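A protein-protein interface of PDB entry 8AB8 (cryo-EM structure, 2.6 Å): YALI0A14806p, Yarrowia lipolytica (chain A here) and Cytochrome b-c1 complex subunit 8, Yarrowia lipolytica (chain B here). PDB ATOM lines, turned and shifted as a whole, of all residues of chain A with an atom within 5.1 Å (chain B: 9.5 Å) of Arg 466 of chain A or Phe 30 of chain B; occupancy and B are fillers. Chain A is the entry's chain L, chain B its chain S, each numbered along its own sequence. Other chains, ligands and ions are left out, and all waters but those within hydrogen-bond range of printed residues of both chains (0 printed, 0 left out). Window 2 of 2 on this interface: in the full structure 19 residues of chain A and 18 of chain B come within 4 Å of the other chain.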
ATOM      1  N   ASP A 445     -20.973 -17.118 -10.204  1.00  0.00           N
ATOM      2  CA  ASP A 445     -22.130 -16.847  -9.353  1.00  0.00           C
ATOM      3  C   ASP A 445     -21.897 -17.344  -7.920  1.00  0.00           C
ATOM      4  O   ASP A 445     -22.785 -17.913  -7.294  1.00  0.00           O
ATOM      5  CB  ASP A 445     -23.395 -17.437  -9.993  1.00  0.00           C
ATOM      6  CG  ASP A 445     -24.714 -17.070  -9.323  1.00  0.00           C
ATOM      7  OD1 ASP A 445     -24.876 -15.897  -8.922  1.00  0.00           O
ATOM      8  OD2 ASP A 445     -25.575 -17.966  -9.203  1.00  0.00           O
ATOM      9  N   LYS A 446     -20.681 -17.180  -7.402  1.00  0.00           N
ATOM     10  CA  LYS A 446     -20.370 -17.694  -6.077  1.00  0.00           C
ATOM     11  C   LYS A 446     -20.162 -16.529  -5.122  1.00  0.00           C
ATOM     12  O   LYS A 446     -19.942 -15.408  -5.559  1.00  0.00           O
ATOM     13  CB  LYS A 446     -19.119 -18.572  -6.117  1.00  0.00           C
ATOM     14  CG  LYS A 446     -19.288 -19.914  -6.813  1.00  0.00           C
ATOM     15  CD  LYS A 446     -20.179 -20.873  -6.060  1.00  0.00           C
ATOM     16  CE  LYS A 446     -19.402 -21.878  -5.240  1.00  0.00           C
ATOM     17  NZ  LYS A 446     -20.296 -22.736  -4.427  1.00  0.00           N
ATOM     18  N   ASP A 447     -20.238 -16.814  -3.818  1.00  0.00           N
ATOM     19  CA  ASP A 447     -19.996 -15.818  -2.790  1.00  0.00           C
ATOM     20  C   ASP A 447     -18.508 -15.506  -2.743  1.00  0.00           C
ATOM     21  O   ASP A 447     -17.684 -16.401  -2.921  1.00  0.00           O
ATOM     22  CB  ASP A 447     -20.366 -16.369  -1.418  1.00  0.00           C
ATOM     23  CG  ASP A 447     -21.815 -16.118  -1.060  1.00  0.00           C
ATOM     24  OD1 ASP A 447     -22.490 -15.382  -1.813  1.00  0.00           O
ATOM     25  OD2 ASP A 447     -22.259 -16.652  -0.020  1.00  0.00           O
ATOM     26  N   ILE A 448     -18.176 -14.252  -2.456  1.00  0.00           N
ATOM     27  CA  ILE A 448     -16.779 -13.887  -2.358  1.00  0.00           C
ATOM     28  C   ILE A 448     -16.516 -13.435  -0.933  1.00  0.00           C
ATOM     29  O   ILE A 448     -17.429 -13.047  -0.216  1.00  0.00           O
ATOM     30  CB  ILE A 448     -16.487 -12.755  -3.346  1.00  0.00           C
ATOM     31  CG1 ILE A 448     -17.531 -11.658  -3.133  1.00  0.00           C
ATOM     32  CG2 ILE A 448     -16.477 -13.290  -4.769  1.00  0.00           C
ATOM     33  CD1 ILE A 448     -17.333 -10.438  -3.970  1.00  0.00           C
ATOM     34  N   TYR A 462     -21.460  -4.930  -1.030  1.00  0.00           N
ATOM     35  CA  TYR A 462     -21.316  -6.349  -1.304  1.00  0.00           C
ATOM     36  C   TYR A 462     -22.107  -6.798  -2.536  1.00  0.00           C
ATOM     37  O   TYR A 462     -21.529  -7.470  -3.382  1.00  0.00           O
ATOM     38  CB  TYR A 462     -21.603  -7.210  -0.072  1.00  0.00           C
ATOM     39  CG  TYR A 462     -21.187  -8.647  -0.256  1.00  0.00           C
ATOM     40  CD1 TYR A 462     -22.061  -9.573  -0.817  1.00  0.00           C
ATOM     41  CD2 TYR A 462     -19.916  -9.085   0.100  1.00  0.00           C
ATOM     42  CE1 TYR A 462     -21.688 -10.893  -1.025  1.00  0.00           C
ATOM     43  CE2 TYR A 462     -19.527 -10.407  -0.099  1.00  0.00           C
ATOM     44  CZ  TYR A 462     -20.415 -11.315  -0.663  1.00  0.00           C
ATOM     45  OH  TYR A 462     -20.049 -12.623  -0.867  1.00  0.00           O
ATOM     46  N   ASN A 463     -23.406  -6.472  -2.625  1.00  0.00           N
ATOM     47  CA  ASN A 463     -24.253  -6.981  -3.700  1.00  0.00           C
ATOM     48  C   ASN A 463     -23.715  -6.588  -5.068  1.00  0.00           C
ATOM     49  O   ASN A 463     -23.584  -7.427  -5.944  1.00  0.00           O
ATOM     50  CB  ASN A 463     -25.695  -6.490  -3.618  1.00  0.00           C
ATOM     51  CG  ASN A 463     -26.497  -7.263  -2.601  1.00  0.00           C
ATOM     52  OD1 ASN A 463     -26.377  -8.480  -2.499  1.00  0.00           O
ATOM     53  ND2 ASN A 463     -27.310  -6.563  -1.838  1.00  0.00           N
ATOM     54  N   ARG A 464     -23.364  -5.318  -5.245  1.00  0.00           N
ATOM     55  CA  ARG A 464     -22.895  -4.886  -6.551  1.00  0.00           C
ATOM     56  C   ARG A 464     -21.586  -5.571  -6.935  1.00  0.00           C
ATOM     57  O   ARG A 464     -21.381  -5.850  -8.116  1.00  0.00           O
ATOM     58  CB  ARG A 464     -22.837  -3.366  -6.629  1.00  0.00           C
ATOM     59  CG  ARG A 464     -24.223  -2.743  -6.708  1.00  0.00           C
ATOM     60  CD  ARG A 464     -24.247  -1.314  -7.212  1.00  0.00           C
ATOM     61  NE  ARG A 464     -23.796  -1.201  -8.590  1.00  0.00           N
ATOM     62  CZ  ARG A 464     -23.484  -0.056  -9.190  1.00  0.00           C
ATOM     63  NH1 ARG A 464     -23.579   1.090  -8.538  1.00  0.00           N
ATOM     64  NH2 ARG A 464     -23.059  -0.063 -10.442  1.00  0.00           N
ATOM     65  N   ILE A 465     -20.721  -5.857  -5.952  1.00  0.00           N
ATOM     66  CA  ILE A 465     -19.516  -6.620  -6.244  1.00  0.00           C
ATOM     67  C   ILE A 465     -19.914  -8.043  -6.619  1.00  0.00           C
ATOM     68  O   ILE A 465     -19.519  -8.538  -7.667  1.00  0.00           O
ATOM     69  CB  ILE A 465     -18.466  -6.611  -5.108  1.00  0.00           C
ATOM     70  CG1 ILE A 465     -18.098  -5.221  -4.570  1.00  0.00           C
ATOM     71  CG2 ILE A 465     -17.236  -7.402  -5.526  1.00  0.00           C
ATOM     72  CD1 ILE A 465     -17.954  -4.130  -5.607  1.00  0.00           C
ATOM     73  N   ARG A 466     -20.693  -8.691  -5.758  1.00  0.00           N
ATOM     74  CA  ARG A 466     -21.075 -10.072  -5.980  1.00  0.00           C
ATOM     75  C   ARG A 466     -21.891 -10.251  -7.259  1.00  0.00           C
ATOM     76  O   ARG A 466     -21.853 -11.318  -7.853  1.00  0.00           O
ATOM     77  CB  ARG A 466     -21.897 -10.568  -4.798  1.00  0.00           C
ATOM     78  CG  ARG A 466     -21.927 -12.082  -4.739  1.00  0.00           C
ATOM     79  CD  ARG A 466     -23.351 -12.552  -4.647  1.00  0.00           C
ATOM     80  NE  ARG A 466     -23.314 -13.979  -4.376  1.00  0.00           N
ATOM     81  CZ  ARG A 466     -23.534 -14.930  -5.278  1.00  0.00           C
ATOM     82  NH1 ARG A 466     -23.817 -14.613  -6.532  1.00  0.00           N
ATOM     83  NH2 ARG A 466     -23.484 -16.196  -4.904  1.00  0.00           N
ATOM     84  N   ASN A 467     -22.616  -9.223  -7.707  1.00  0.00           N
ATOM     85  CA  ASN A 467     -23.341  -9.348  -8.963  1.00  0.00           C
ATOM     86  C   ASN A 467     -22.406  -9.458 -10.168  1.00  0.00           C
ATOM     87  O   ASN A 467     -22.806  -9.972 -11.211  1.00  0.00           O
ATOM     88  CB  ASN A 467     -24.330  -8.209  -9.176  1.00  0.00           C
ATOM     89  CG  ASN A 467     -25.451  -8.223  -8.160  1.00  0.00           C
ATOM     90  OD1 ASN A 467     -25.711  -9.243  -7.520  1.00  0.00           O
ATOM     91  ND2 ASN A 467     -26.102  -7.083  -7.985  1.00  0.00           N
ATOM     92  N   ASP A 468     -21.166  -8.981 -10.044  1.00  0.00           N
ATOM     93  CA  ASP A 468     -20.215  -9.172 -11.127  1.00  0.00           C
ATOM     94  C   ASP A 468     -19.673 -10.597 -11.213  1.00  0.00           C
ATOM     95  O   ASP A 468     -18.890 -10.891 -12.113  1.00  0.00           O
ATOM     96  CB  ASP A 468     -19.117  -8.112 -11.128  1.00  0.00           C
ATOM     97  CG  ASP A 468     -19.590  -6.833 -11.791  1.00  0.00           C
ATOM     98  OD1 ASP A 468     -20.551  -6.906 -12.586  1.00  0.00           O
ATOM     99  OD2 ASP A 468     -19.028  -5.766 -11.475  1.00  0.00           O
ATOM    100  N   MET A 469     -20.087 -11.491 -10.312  1.00  0.00           N
ATOM    101  CA  MET A 469     -19.609 -12.865 -10.389  1.00  0.00           C
ATOM    102  C   MET A 469     -20.372 -13.672 -11.437  1.00  0.00           C
ATOM    103  O   MET A 469     -20.140 -14.869 -11.567  1.00  0.00           O
ATOM    104  CB  MET A 469     -19.683 -13.589  -9.044  1.00  0.00           C
ATOM    105  CG  MET A 469     -18.794 -12.967  -7.989  1.00  0.00           C
ATOM    106  SD  MET A 469     -17.028 -13.056  -8.421  1.00  0.00           S
ATOM    107  CE  MET A 469     -16.658 -14.771  -8.063  1.00  0.00           C
ATOM    108  N   SER A 470     -21.284 -13.036 -12.172  1.00  0.00           N
ATOM    109  CA  SER A 470     -21.926 -13.736 -13.272  1.00  0.00           C
ATOM    110  C   SER A 470     -22.173 -12.740 -14.389  1.00  0.00           C
ATOM    111  O   SER A 470     -22.021 -11.547 -14.185  1.00  0.00           O
ATOM    112  CB  SER A 470     -23.196 -14.404 -12.829  1.00  0.00           C
ATOM    113  OG  SER A 470     -24.041 -13.468 -12.185  1.00  0.00           O
ATOM    114  N   ILE B  27     -22.296  -9.947   5.869  1.00  0.00           N
ATOM    115  CA  ILE B  27     -22.245 -11.237   5.213  1.00  0.00           C
ATOM    116  C   ILE B  27     -23.116 -11.206   3.963  1.00  0.00           C
ATOM    117  O   ILE B  27     -24.027 -10.389   3.846  1.00  0.00           O
ATOM    118  CB  ILE B  27     -22.661 -12.349   6.191  1.00  0.00           C
ATOM    119  CG1 ILE B  27     -24.095 -12.140   6.678  1.00  0.00           C
ATOM    120  CG2 ILE B  27     -21.668 -12.454   7.346  1.00  0.00           C
ATOM    121  CD1 ILE B  27     -24.697 -13.342   7.386  1.00  0.00           C
ATOM    122  N   SER B  28     -22.845 -12.153   3.064  1.00  0.00           N
ATOM    123  CA  SER B  28     -23.505 -12.313   1.782  1.00  0.00           C
ATOM    124  C   SER B  28     -25.014 -12.501   1.950  1.00  0.00           C
ATOM    125  O   SER B  28     -25.452 -13.124   2.909  1.00  0.00           O
ATOM    126  CB  SER B  28     -22.892 -13.498   1.102  1.00  0.00           C
ATOM    127  OG  SER B  28     -23.614 -13.854  -0.062  1.00  0.00           O
ATOM    128  N   PRO B  29     -25.866 -12.012   1.017  1.00  0.00           N
ATOM    129  CA  PRO B  29     -27.296 -12.322   1.053  1.00  0.00           C
ATOM    130  C   PRO B  29     -27.564 -13.823   1.003  1.00  0.00           C
ATOM    131  O   PRO B  29     -28.526 -14.284   1.606  1.00  0.00           O
ATOM    132  CB  PRO B  29     -27.865 -11.639  -0.201  1.00  0.00           C
ATOM    133  CG  PRO B  29     -26.668 -11.446  -1.090  1.00  0.00           C
ATOM    134  CD  PRO B  29     -25.525 -11.167  -0.138  1.00  0.00           C
ATOM    135  N   PHE B  30     -26.710 -14.582   0.304  1.00  0.00           N
ATOM    136  CA  PHE B  30     -26.890 -16.028   0.244  1.00  0.00           C
ATOM    137  C   PHE B  30     -26.487 -16.720   1.545  1.00  0.00           C
ATOM    138  O   PHE B  30     -26.894 -17.854   1.791  1.00  0.00           O
ATOM    139  CB  PHE B  30     -26.143 -16.642  -0.939  1.00  0.00           C
ATOM    140  CG  PHE B  30     -26.706 -16.262  -2.283  1.00  0.00           C
ATOM    141  CD1 PHE B  30     -27.680 -17.043  -2.897  1.00  0.00           C
ATOM    142  CD2 PHE B  30     -26.270 -15.113  -2.934  1.00  0.00           C
ATOM    143  CE1 PHE B  30     -28.191 -16.690  -4.140  1.00  0.00           C
ATOM    144  CE2 PHE B  30     -26.786 -14.756  -4.175  1.00  0.00           C
ATOM    145  CZ  PHE B  30     -27.747 -15.546  -4.777  1.00  0.00           C
ATOM    146  N   ALA B  31     -25.685 -16.049   2.375  1.00  0.00           N
ATOM    147  CA  ALA B  31     -25.235 -16.673   3.609  1.00  0.00           C
ATOM    148  C   ALA B  31     -26.198 -16.370   4.755  1.00  0.00           C
ATOM    149  O   ALA B  31     -26.100 -16.976   5.821  1.00  0.00           O
ATOM    150  CB  ALA B  31     -23.830 -16.230   3.929  1.00  0.00           C
ATOM    151  N   ALA B  32     -27.099 -15.409   4.541  1.00  0.00           N
ATOM    152  CA  ALA B  32     -27.949 -14.932   5.619  1.00  0.00           C
ATOM    153  C   ALA B  32     -29.352 -15.512   5.508  1.00  0.00           C
ATOM    154  O   ALA B  32     -29.825 -15.824   4.418  1.00  0.00           O
ATOM    155  CB  ALA B  32     -27.985 -13.428   5.614  1.00  0.00           C
ATOM    156  N   ARG B  33     -30.025 -15.622   6.652  1.00  0.00           N
ATOM    157  CA  ARG B  33     -31.456 -15.869   6.644  1.00  0.00           C
ATOM    158  C   ARG B  33     -32.177 -14.528   6.529  1.00  0.00           C
ATOM    159  O   ARG B  33     -32.192 -13.753   7.483  1.00  0.00           O
ATOM    160  CB  ARG B  33     -31.852 -16.582   7.935  1.00  0.00           C
ATOM    161  CG  ARG B  33     -31.292 -17.988   8.075  1.00  0.00           C
ATOM    162  CD  ARG B  33     -31.815 -18.602   9.361  1.00  0.00           C
ATOM    163  NE  ARG B  33     -31.058 -18.107  10.502  1.00  0.00           N
ATOM    164  CZ  ARG B  33     -29.978 -18.701  10.998  1.00  0.00           C
ATOM    165  NH1 ARG B  33     -29.536 -19.832  10.470  1.00  0.00           N
ATOM    166  NH2 ARG B  33     -29.349 -18.172  12.033  1.00  0.00           N
ATOM    167  N   PRO B  34     -32.823 -14.197   5.388  1.00  0.00           N
ATOM    168  CA  PRO B  34     -33.411 -12.870   5.213  1.00  0.00           C
ATOM    169  C   PRO B  34     -34.499 -12.571   6.239  1.00  0.00           C
ATOM    170  O   PRO B  34     -34.667 -11.422   6.641  1.00  0.00           O
ATOM    171  CB  PRO B  34     -34.056 -12.883   3.827  1.00  0.00           C
ATOM    172  CG  PRO B  34     -33.548 -14.135   3.159  1.00  0.00           C
ATOM    173  CD  PRO B  34     -33.065 -15.076   4.237  1.00  0.00           C
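The side-chain hydroxyl of Ser 28 of chain B lies within hydrogen-bond range of the side-chain carboxylate of Asp 447 of chain A (2.6 Å).
Among the printed residues, merely in contact across the chains: Asn 463 of chain A with Pro 29 of chain B (3.3 Å), Arg 466 of chain A with Phe 30 of chain B (3.4 Å), Tyr 462 of chain A with Ser 28 of chain B (3.6 Å), Tyr 462 of chain A with Pro 29 of chain B (3.9 Å) and Asp 447 of chain A with Phe 30 of chain B (3.95 Å).
The backbone carbonyl oxygen of Ile 448 of chain A is in hydrogen-bond range of the side-chain hydroxyl of Tyr 462 of chain A, at 2.7 Å. The side-chain carboxylate of Asp 447 of chain A is in salt-bridge range of the guanidinium group of Arg 466 of chain A, 3.0 Å away. O of Asn 463 of chain A lies close to OD1 of Asn 467 of chain A. The guanidinium group (NH1) of Arg 466 of chain A lies within salt-bridge range of the side-chain carboxylate (OD1) of Asp 445 of chain A (2.9 Å). The backbone NH (N) of Phe 30 of chain B sits close to the side-chain hydroxyl (OG) of Ser 28 of chain B.
Of the printed residues of chain B, Arg 466 of chain A touches Phe 30. No residue of chain B comes within 4 Å of Asp 445 of chain A. No residue of chain B comes within 4 Å of Ile 465 of chain A. No residue of chain B comes within 4 Å of Asn 467 of chain A. Printed residues of chain B within 4 Å of Asp 447 of chain A: Ser 28 and Phe 30. Of the printed residues of chain B, Asn 463 of chain A touches Pro 29. Printed residues of chain B within 4 Å of Tyr 462 of chain A: Ser 28 and Pro 29. The nearest printed residue of chain A that does not touch Phe 30 of chain B is Asp 445 of chain A (5.1 Å).
Of the 13 printed residues of chain A, 4 touch a printed residue of chain B. Among the printed residues, no Asp or Glu carboxylate lies within 4 Å of a Lys or Arg side-chain nitrogen of the other chain.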
